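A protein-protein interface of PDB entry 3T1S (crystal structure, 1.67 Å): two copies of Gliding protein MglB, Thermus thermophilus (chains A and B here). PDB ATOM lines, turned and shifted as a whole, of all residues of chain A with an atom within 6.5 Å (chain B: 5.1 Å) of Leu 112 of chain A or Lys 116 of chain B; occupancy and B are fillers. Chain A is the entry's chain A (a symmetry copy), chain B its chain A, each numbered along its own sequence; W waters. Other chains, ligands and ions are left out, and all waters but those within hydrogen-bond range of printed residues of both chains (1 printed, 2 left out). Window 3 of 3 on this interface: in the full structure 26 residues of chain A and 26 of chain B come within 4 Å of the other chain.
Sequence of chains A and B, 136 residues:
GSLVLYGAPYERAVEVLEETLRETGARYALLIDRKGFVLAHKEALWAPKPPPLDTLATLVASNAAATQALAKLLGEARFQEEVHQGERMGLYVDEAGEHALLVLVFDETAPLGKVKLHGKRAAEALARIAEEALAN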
ATOM      1  N   VAL A  83      13.101   6.577  -0.972  1.00  0.00           N
ATOM      2  CA  VAL A  83      12.796   6.793  -2.422  1.00  0.00           C
ATOM      3  C   VAL A  83      13.997   6.309  -3.195  1.00  0.00           C
ATOM      4  O   VAL A  83      15.178   6.647  -2.844  1.00  0.00           O
ATOM      5  CB  VAL A  83      12.563   8.250  -2.709  1.00  0.00           C
ATOM      6  CG1 VAL A  83      12.419   8.406  -4.243  1.00  0.00           C
ATOM      7  CG2 VAL A  83      11.173   8.724  -2.089  1.00  0.00           C
ATOM      8  N   GLN A  85      15.449   6.299  -7.142  1.00  0.00           N
ATOM      9  CA  GLN A  85      15.081   6.827  -8.507  1.00  0.00           C
ATOM     10  C   GLN A  85      16.072   6.396  -9.559  1.00  0.00           C
ATOM     11  O   GLN A  85      17.303   6.477  -9.383  1.00  0.00           O
ATOM     12  CB  GLN A  85      14.944   8.341  -8.566  1.00  0.00           C
ATOM     13  CG  GLN A  85      13.925   8.875  -7.590  1.00  0.00           C
ATOM     14  CD  GLN A  85      13.662  10.314  -7.817  1.00  0.00           C
ATOM     15  OE1 GLN A  85      13.097  10.657  -8.869  1.00  0.00           O
ATOM     16  NE2 GLN A  85      14.032  11.179  -6.868  1.00  0.00           N
ATOM     17  N   TYR A  92       8.963   4.102  -4.197  1.00  0.00           N
ATOM     18  CA  TYR A  92       8.695   4.819  -2.948  1.00  0.00           C
ATOM     19  C   TYR A  92       8.230   3.791  -1.917  1.00  0.00           C
ATOM     20  O   TYR A  92       7.326   2.948  -2.203  1.00  0.00           O
ATOM     21  CB  TYR A  92       7.647   5.901  -3.200  1.00  0.00           C
ATOM     22  CG  TYR A  92       7.048   6.508  -1.966  1.00  0.00           C
ATOM     23  CD1 TYR A  92       7.617   7.624  -1.366  1.00  0.00           C
ATOM     24  CD2 TYR A  92       5.845   5.998  -1.429  1.00  0.00           C
ATOM     25  CE1 TYR A  92       6.982   8.210  -0.193  1.00  0.00           C
ATOM     26  CE2 TYR A  92       5.237   6.558  -0.322  1.00  0.00           C
ATOM     27  CZ  TYR A  92       5.796   7.675   0.255  1.00  0.00           C
ATOM     28  OH  TYR A  92       5.183   8.199   1.362  1.00  0.00           O
ATOM     29  N   PHE A 106       6.637   3.959  -9.764  1.00  0.00           N
ATOM     30  CA  PHE A 106       6.159   5.034 -10.650  1.00  0.00           C
ATOM     31  C   PHE A 106       7.193   5.370 -11.712  1.00  0.00           C
ATOM     32  O   PHE A 106       8.312   4.888 -11.681  1.00  0.00           O
ATOM     33  CB  PHE A 106       5.830   6.254  -9.805  1.00  0.00           C
ATOM     34  CG  PHE A 106       7.031   6.790  -9.009  1.00  0.00           C
ATOM     35  CD1 PHE A 106       7.790   7.851  -9.523  1.00  0.00           C
ATOM     36  CD2 PHE A 106       7.426   6.228  -7.767  1.00  0.00           C
ATOM     37  CE1 PHE A 106       8.902   8.364  -8.822  1.00  0.00           C
ATOM     38  CE2 PHE A 106       8.543   6.713  -7.098  1.00  0.00           C
ATOM     39  CZ  PHE A 106       9.323   7.747  -7.637  1.00  0.00           C
ATOM     40  N   GLU A 108       8.294   8.724 -14.839  1.00  0.00           N
ATOM     41  CA  GLU A 108       8.457  10.194 -14.878  1.00  0.00           C
ATOM     42  C   GLU A 108       7.191  11.018 -14.983  1.00  0.00           C
ATOM     43  O   GLU A 108       7.201  12.248 -14.702  1.00  0.00           O
ATOM     44  CB  GLU A 108       9.375  10.599 -16.040  1.00  0.00           C
ATOM     45  CG  GLU A 108       8.751  10.413 -17.443  1.00  0.00           C
ATOM     46  CD  GLU A 108       9.769  10.653 -18.526  1.00  0.00           C
ATOM     47  OE1 GLU A 108      10.889  11.127 -18.199  1.00  0.00           O
ATOM     48  OE2 GLU A 108       9.474  10.332 -19.690  1.00  0.00           O
ATOM     49  N   ALA A 110       4.661  10.569 -13.137  1.00  0.00           N
ATOM     50  CA  ALA A 110       4.161  10.770 -11.805  1.00  0.00           C
ATOM     51  C   ALA A 110       5.108  11.723 -11.056  1.00  0.00           C
ATOM     52  O   ALA A 110       6.232  11.314 -10.764  1.00  0.00           O
ATOM     53  CB  ALA A 110       4.165   9.430 -11.077  1.00  0.00           C
ATOM     54  N   PRO A 111       4.651  12.932 -10.729  1.00  0.00           N
ATOM     55  CA  PRO A 111       5.362  14.017 -10.028  1.00  0.00           C
ATOM     56  C   PRO A 111       5.794  13.461  -8.684  1.00  0.00           C
ATOM     57  O   PRO A 111       4.924  12.971  -7.914  1.00  0.00           O
ATOM     58  CB  PRO A 111       4.266  15.043  -9.741  1.00  0.00           C
ATOM     59  CG  PRO A 111       3.279  14.825 -10.813  1.00  0.00           C
ATOM     60  CD  PRO A 111       3.290  13.351 -11.141  1.00  0.00           C
ATOM     61  N   LEU A 112       7.085  13.475  -8.420  1.00  0.00           N
ATOM     62  CA  LEU A 112       7.534  12.861  -7.109  1.00  0.00           C
ATOM     63  C   LEU A 112       6.893  13.531  -5.915  1.00  0.00           C
ATOM     64  O   LEU A 112       6.593  12.885  -4.904  1.00  0.00           O
ATOM     65  CB  LEU A 112       9.082  12.911  -6.951  1.00  0.00           C
ATOM     66  CG  LEU A 112       9.642  12.329  -5.638  1.00  0.00           C
ATOM     67  CD1 LEU A 112       9.440  10.813  -5.622  1.00  0.00           C
ATOM     68  CD2 LEU A 112      11.148  12.607  -5.465  1.00  0.00           C
ATOM     69  N   GLY A 113       6.664  14.841  -5.972  1.00  0.00           N
ATOM     70  CA  GLY A 113       5.998  15.500  -4.891  1.00  0.00           C
ATOM     71  C   GLY A 113       4.616  14.922  -4.605  1.00  0.00           C
ATOM     72  O   GLY A 113       4.252  14.755  -3.450  1.00  0.00           O
ATOM     73  N   LYS A 114       3.865  14.624  -5.669  1.00  0.00           N
ATOM     74  CA  LYS A 114       2.517  14.000  -5.506  1.00  0.00           C
ATOM     75  C   LYS A 114       2.663  12.581  -4.964  1.00  0.00           C
ATOM     76  O   LYS A 114       1.872  12.167  -4.091  1.00  0.00           O
ATOM     77  CB  LYS A 114       1.768  13.927  -6.845  1.00  0.00           C
ATOM     78  CG  LYS A 114       0.818  15.069  -7.035  1.00  0.00           C
ATOM     79  CD  LYS A 114       0.283  15.019  -8.481  1.00  0.00           C
ATOM     80  CE  LYS A 114      -0.243  16.387  -8.865  1.00  0.00           C
ATOM     81  NZ  LYS A 114       0.054  16.727 -10.305  1.00  0.00           N
ATOM     82  N   VAL A 115       3.630  11.846  -5.489  1.00  0.00           N
ATOM     83  CA  VAL A 115       3.857  10.482  -5.005  1.00  0.00           C
ATOM     84  C   VAL A 115       4.111  10.504  -3.515  1.00  0.00           C
ATOM     85  O   VAL A 115       3.528   9.723  -2.766  1.00  0.00           O
ATOM     86  CB  VAL A 115       5.012   9.819  -5.728  1.00  0.00           C
ATOM     87  CG1 VAL A 115       5.441   8.545  -4.988  1.00  0.00           C
ATOM     88  CG2 VAL A 115       4.687   9.602  -7.284  1.00  0.00           C
ATOM     89  N   LYS A 116       5.018  11.387  -3.029  1.00  0.00           N
ATOM     90  CA  LYS A 116       5.278  11.481  -1.604  1.00  0.00           C
ATOM     91  C   LYS A 116       4.082  11.980  -0.746  1.00  0.00           C
ATOM     92  O   LYS A 116       3.803  11.428   0.328  1.00  0.00           O
ATOM     93  CB  LYS A 116       6.562  12.348  -1.365  1.00  0.00           C
ATOM     94  CG  LYS A 116       7.789  11.557  -1.792  1.00  0.00           C
ATOM     95  CD  LYS A 116       9.129  12.374  -1.843  1.00  0.00           C
ATOM     96  CE  LYS A 116       9.623  12.743  -0.519  1.00  0.00           C
ATOM     97  NZ  LYS A 116      10.747  13.700  -0.755  1.00  0.00           N
ATOM     98  N   LEU A 117       3.378  13.003  -1.253  1.00  0.00           N
ATOM     99  CA  LEU A 117       2.314  13.640  -0.513  1.00  0.00           C
ATOM    100  C   LEU A 117       1.139  12.698  -0.334  1.00  0.00           C
ATOM    101  O   LEU A 117       0.673  12.490   0.779  1.00  0.00           O
ATOM    102  CB  LEU A 117       1.805  14.826  -1.274  1.00  0.00           C
ATOM    103  CG  LEU A 117       0.886  15.820  -0.595  1.00  0.00           C
ATOM    104  CD1 LEU A 117       1.126  15.846   0.876  1.00  0.00           C
ATOM    105  CD2 LEU A 117       1.340  17.131  -1.182  1.00  0.00           C
ATOM    106  N   GLU B  81      19.865   7.429  -7.756  1.00  0.00           N
ATOM    107  CA  GLU B  81      19.795   8.289  -6.558  1.00  0.00           C
ATOM    108  C   GLU B  81      18.893   7.594  -5.528  1.00  0.00           C
ATOM    109  O   GLU B  81      17.936   6.943  -5.920  1.00  0.00           O
ATOM    110  CB  GLU B  81      19.280   9.667  -6.934  1.00  0.00           C
ATOM    111  CG  GLU B  81      19.341  10.760  -5.844  1.00  0.00           C
ATOM    112  CD  GLU B  81      17.975  10.986  -5.169  1.00  0.00           C
ATOM    113  OE1 GLU B  81      17.497  12.107  -5.160  1.00  0.00           O
ATOM    114  OE2 GLU B  81      17.349  10.040  -4.692  1.00  0.00           O
ATOM    115  N   VAL B  83      17.094   8.238  -1.371  1.00  0.00           N
ATOM    116  CA  VAL B  83      16.943   9.067  -0.133  1.00  0.00           C
ATOM    117  C   VAL B  83      16.346   8.168   0.920  1.00  0.00           C
ATOM    118  O   VAL B  83      15.341   7.426   0.651  1.00  0.00           O
ATOM    119  CB  VAL B  83      16.030  10.235  -0.378  1.00  0.00           C
ATOM    120  CG1 VAL B  83      15.799  10.939   0.982  1.00  0.00           C
ATOM    121  CG2 VAL B  83      16.743  11.313  -1.312  1.00  0.00           C
ATOM    122  N   TYR B  92      21.243  10.689   1.858  1.00  0.00           N
ATOM    123  CA  TYR B  92      21.099  10.914   0.419  1.00  0.00           C
ATOM    124  C   TYR B  92      22.297  10.264  -0.272  1.00  0.00           C
ATOM    125  O   TYR B  92      23.478  10.473   0.142  1.00  0.00           O
ATOM    126  CB  TYR B  92      21.020  12.417   0.147  1.00  0.00           C
ATOM    127  CG  TYR B  92      21.180  12.813  -1.291  1.00  0.00           C
ATOM    128  CD1 TYR B  92      20.083  12.909  -2.136  1.00  0.00           C
ATOM    129  CD2 TYR B  92      22.450  13.172  -1.796  1.00  0.00           C
ATOM    130  CE1 TYR B  92      20.274  13.339  -3.514  1.00  0.00           C
ATOM    131  CE2 TYR B  92      22.632  13.587  -3.101  1.00  0.00           C
ATOM    132  CZ  TYR B  92      21.536  13.699  -3.927  1.00  0.00           C
ATOM    133  OH  TYR B  92      21.747  14.095  -5.221  1.00  0.00           O
ATOM    134  N   LEU B 112      15.289  19.257   2.447  1.00  0.00           N
ATOM    135  CA  LEU B 112      15.603  18.124   1.491  1.00  0.00           C
ATOM    136  C   LEU B 112      15.742  18.604   0.064  1.00  0.00           C
ATOM    137  O   LEU B 112      16.552  18.081  -0.711  1.00  0.00           O
ATOM    138  CB  LEU B 112      14.521  17.007   1.549  1.00  0.00           C
ATOM    139  CG  LEU B 112      14.736  15.814   0.595  1.00  0.00           C
ATOM    140  CD1 LEU B 112      15.952  15.006   1.050  1.00  0.00           C
ATOM    141  CD2 LEU B 112      13.523  14.864   0.559  1.00  0.00           C
ATOM    142  N   GLY B 113      14.964  19.603  -0.347  1.00  0.00           N
ATOM    143  CA  GLY B 113      15.111  20.131  -1.668  1.00  0.00           C
ATOM    144  C   GLY B 113      16.516  20.656  -1.944  1.00  0.00           C
ATOM    145  O   GLY B 113      17.052  20.430  -3.019  1.00  0.00           O
ATOM    146  N   LYS B 114      17.094  21.351  -0.961  1.00  0.00           N
ATOM    147  CA  LYS B 114      18.490  21.865  -1.100  1.00  0.00           C
ATOM    148  C   LYS B 114      19.473  20.698  -1.119  1.00  0.00           C
ATOM    149  O   LYS B 114      20.438  20.712  -1.911  1.00  0.00           O
ATOM    150  CB  LYS B 114      18.867  22.790   0.066  1.00  0.00           C
ATOM    151  CG  LYS B 114      18.687  24.239  -0.269  1.00  0.00           C
ATOM    152  CD  LYS B 114      18.884  25.062   1.020  1.00  0.00           C
ATOM    153  CE  LYS B 114      18.223  26.415   0.853  1.00  0.00           C
ATOM    154  NZ  LYS B 114      17.570  26.890   2.129  1.00  0.00           N
ATOM    155  N   VAL B 115      19.251  19.725  -0.248  1.00  0.00           N
ATOM    156  CA  VAL B 115      20.131  18.555  -0.219  1.00  0.00           C
ATOM    157  C   VAL B 115      20.154  17.899  -1.580  1.00  0.00           C
ATOM    158  O   VAL B 115      21.217  17.578  -2.106  1.00  0.00           O
ATOM    159  CB  VAL B 115      19.699  17.560   0.840  1.00  0.00           C
ATOM    160  CG1 VAL B 115      20.412  16.217   0.631  1.00  0.00           C
ATOM    161  CG2 VAL B 115      19.854  18.166   2.317  1.00  0.00           C
ATOM    162  N   LYS B 116      18.971  17.646  -2.194  1.00  0.00           N
ATOM    163  CA  LYS B 116      18.930  17.052  -3.518  1.00  0.00           C
ATOM    164  C   LYS B 116      19.525  17.928  -4.655  1.00  0.00           C
ATOM    165  O   LYS B 116      20.263  17.429  -5.516  1.00  0.00           O
ATOM    166  CB  LYS B 116      17.462  16.604  -3.841  1.00  0.00           C
ATOM    167  CG  LYS B 116      17.115  15.381  -3.007  1.00  0.00           C
ATOM    168  CD  LYS B 116      15.602  14.957  -3.036  1.00  0.00           C
ATOM    169  CE  LYS B 116      15.190  14.402  -4.322  1.00  0.00           C
ATOM    170  NZ  LYS B 116      13.701  14.281  -4.254  1.00  0.00           N
ATOM    171  N   LEU B 117      19.213  19.233  -4.619  1.00  0.00           N
ATOM    172  CA  LEU B 117      19.602  20.142  -5.672  1.00  0.00           C
ATOM    173  C   LEU B 117      21.107  20.329  -5.698  1.00  0.00           C
ATOM    174  O   LEU B 117      21.736  20.162  -6.735  1.00  0.00           O
ATOM    175  CB  LEU B 117      19.004  21.493  -5.424  1.00  0.00           C
ATOM    176  CG  LEU B 117      19.031  22.541  -6.516  1.00  0.00           C
ATOM    177  CD1 LEU B 117      19.059  21.903  -7.864  1.00  0.00           C
ATOM    178  CD2 LEU B 117      17.705  23.230  -6.335  1.00  0.00           C
ATOM    179  N   HIS B 118      21.675  20.621  -4.548  1.00  0.00           N
ATOM    180  CA  HIS B 118      23.158  20.772  -4.470  1.00  0.00           C
ATOM    181  C   HIS B 118      23.885  19.433  -4.513  1.00  0.00           C
ATOM    182  O   HIS B 118      25.047  19.367  -4.890  1.00  0.00           O
ATOM    183  CB  HIS B 118      23.550  21.570  -3.229  1.00  0.00           C
ATOM    184  CG  HIS B 118      23.018  22.963  -3.276  1.00  0.00           C
ATOM    185  ND1 HIS B 118      23.486  23.882  -4.191  1.00  0.00           N
ATOM    186  CD2 HIS B 118      22.061  23.599  -2.549  1.00  0.00           C
ATOM    187  CE1 HIS B 118      22.832  25.022  -4.038  1.00  0.00           C
ATOM    188  NE2 HIS B 118      21.970  24.881  -3.047  1.00  0.00           N
ATOM    189  N   GLY B 119      23.228  18.375  -4.048  1.00  0.00           N
ATOM    190  CA  GLY B 119      23.818  17.057  -3.994  1.00  0.00           C
ATOM    191  C   GLY B 119      24.046  16.601  -5.407  1.00  0.00           C
ATOM    192  O   GLY B 119      25.093  16.075  -5.723  1.00  0.00           O
ATOM    193  N   LYS B 120      23.061  16.864  -6.276  1.00  0.00           N
ATOM    194  CA  LYS B 120      23.173  16.446  -7.692  1.00  0.00           C
ATOM    195  C   LYS B 120      24.336  17.190  -8.384  1.00  0.00           C
ATOM    196  O   LYS B 120      25.150  16.560  -9.076  1.00  0.00           O
ATOM    197  CB  LYS B 120      21.840  16.658  -8.448  1.00  0.00           C
ATOM    198  CG  LYS B 120      21.902  16.291  -9.946  1.00  0.00           C
ATOM    199  CD  LYS B 120      20.749  16.955 -10.749  1.00  0.00           C
ATOM    200  CE  LYS B 120      20.995  16.852 -12.257  1.00  0.00           C
ATOM    201  NZ  LYS B 120      19.939  17.544 -13.050  1.00  0.00           N
ATOM    202  N   ARG B 121      24.429  18.508  -8.169  1.00  0.00           N
ATOM    203  CA  ARG B 121      25.499  19.320  -8.724  1.00  0.00           C
ATOM    204  C   ARG B 121      26.824  18.767  -8.211  1.00  0.00           C
ATOM    205  O   ARG B 121      27.750  18.529  -8.994  1.00  0.00           O
ATOM    206  CB  ARG B 121      25.279  20.794  -8.365  1.00  0.00           C
ATOM    207  CG  ARG B 121      24.145  21.402  -9.183  1.00  0.00           C
ATOM    208  CD  ARG B 121      24.008  22.916  -8.849  1.00  0.00           C
ATOM    209  NE  ARG B 121      22.891  23.578  -9.556  1.00  0.00           N
ATOM    210  CZ  ARG B 121      22.964  24.133 -10.778  1.00  0.00           C
ATOM    211  NH1 ARG B 121      24.121  24.146 -11.439  1.00  0.00           N
ATOM    212  NH2 ARG B 121      21.884  24.724 -11.331  1.00  0.00           N
HETATM  213  O   HOH W   1      14.833  10.663  -4.328  1.00  0.00           O
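The backbone carbonyl oxygen of Val 83 of chain B lies within hydrogen-bond range of the backbone NH of Val 83 of chain A, 2.9 Å away.
The backbone carbonyl oxygen of Glu 81 of chain B is in hydrogen-bond range of the backbone NH of Gln 85 of chain A, at 2.8 Å.
Among the printed residues, merely in contact across the chains: Leu 112 of chain A with Lys 116 of chain B (3.3 Å) and Lys 116 of chain A with Leu 112 of chain B (3.3 Å).
Of chain A, only Leu 112 (3.3 Å) comes within 4 Å of Lys 116 of chain B.
Printed residues of chain B within 4 Å of Val 83 of chain A: Val 83.
Of the printed residues of chain A, Leu 112 of chain B touches Lys 116 (3.3 Å).
Of the printed residues of chain A, Val 83 of chain B touches Val 83 (2.9 Å).
Printed residues of chain B within 4 Å of Lys 116 of chain A: Leu 112 (3.3 Å).
Arg 121 of chain B touches none of the printed residues of chain A.
The nearest printed residue of chain B that does not touch Gln 85 of chain A is Lys 116 of chain B (4.1 Å).
Of the 13 printed residues of chain A, 4 touch a printed residue of chain B.
Along chain B the printed residues that touch a printed residue of chain A span positions 81 to 116.
Among the printed residues, 4 pairs touch across the chains.
Among the printed residues, no Asp or Glu carboxylate lies within 4 Å of a Lys or Arg side-chain nitrogen of the other chain.
Val 83 of chain A touches its own counterpart, Val 83 of chain B.
Leu 112 of chain A touches Lys 116 of chain B, and with the chains exchanged Lys 116 of chain A touches Leu 112 of chain B.
Positions printed for both chains: 83, 92, 112, 113, 114, 115, 116 and 117.
Water W1 bridges OE2 of Glu 81 of chain B (2.6 Å) and NE2 of Gln 85 of chain A (2.7 Å).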
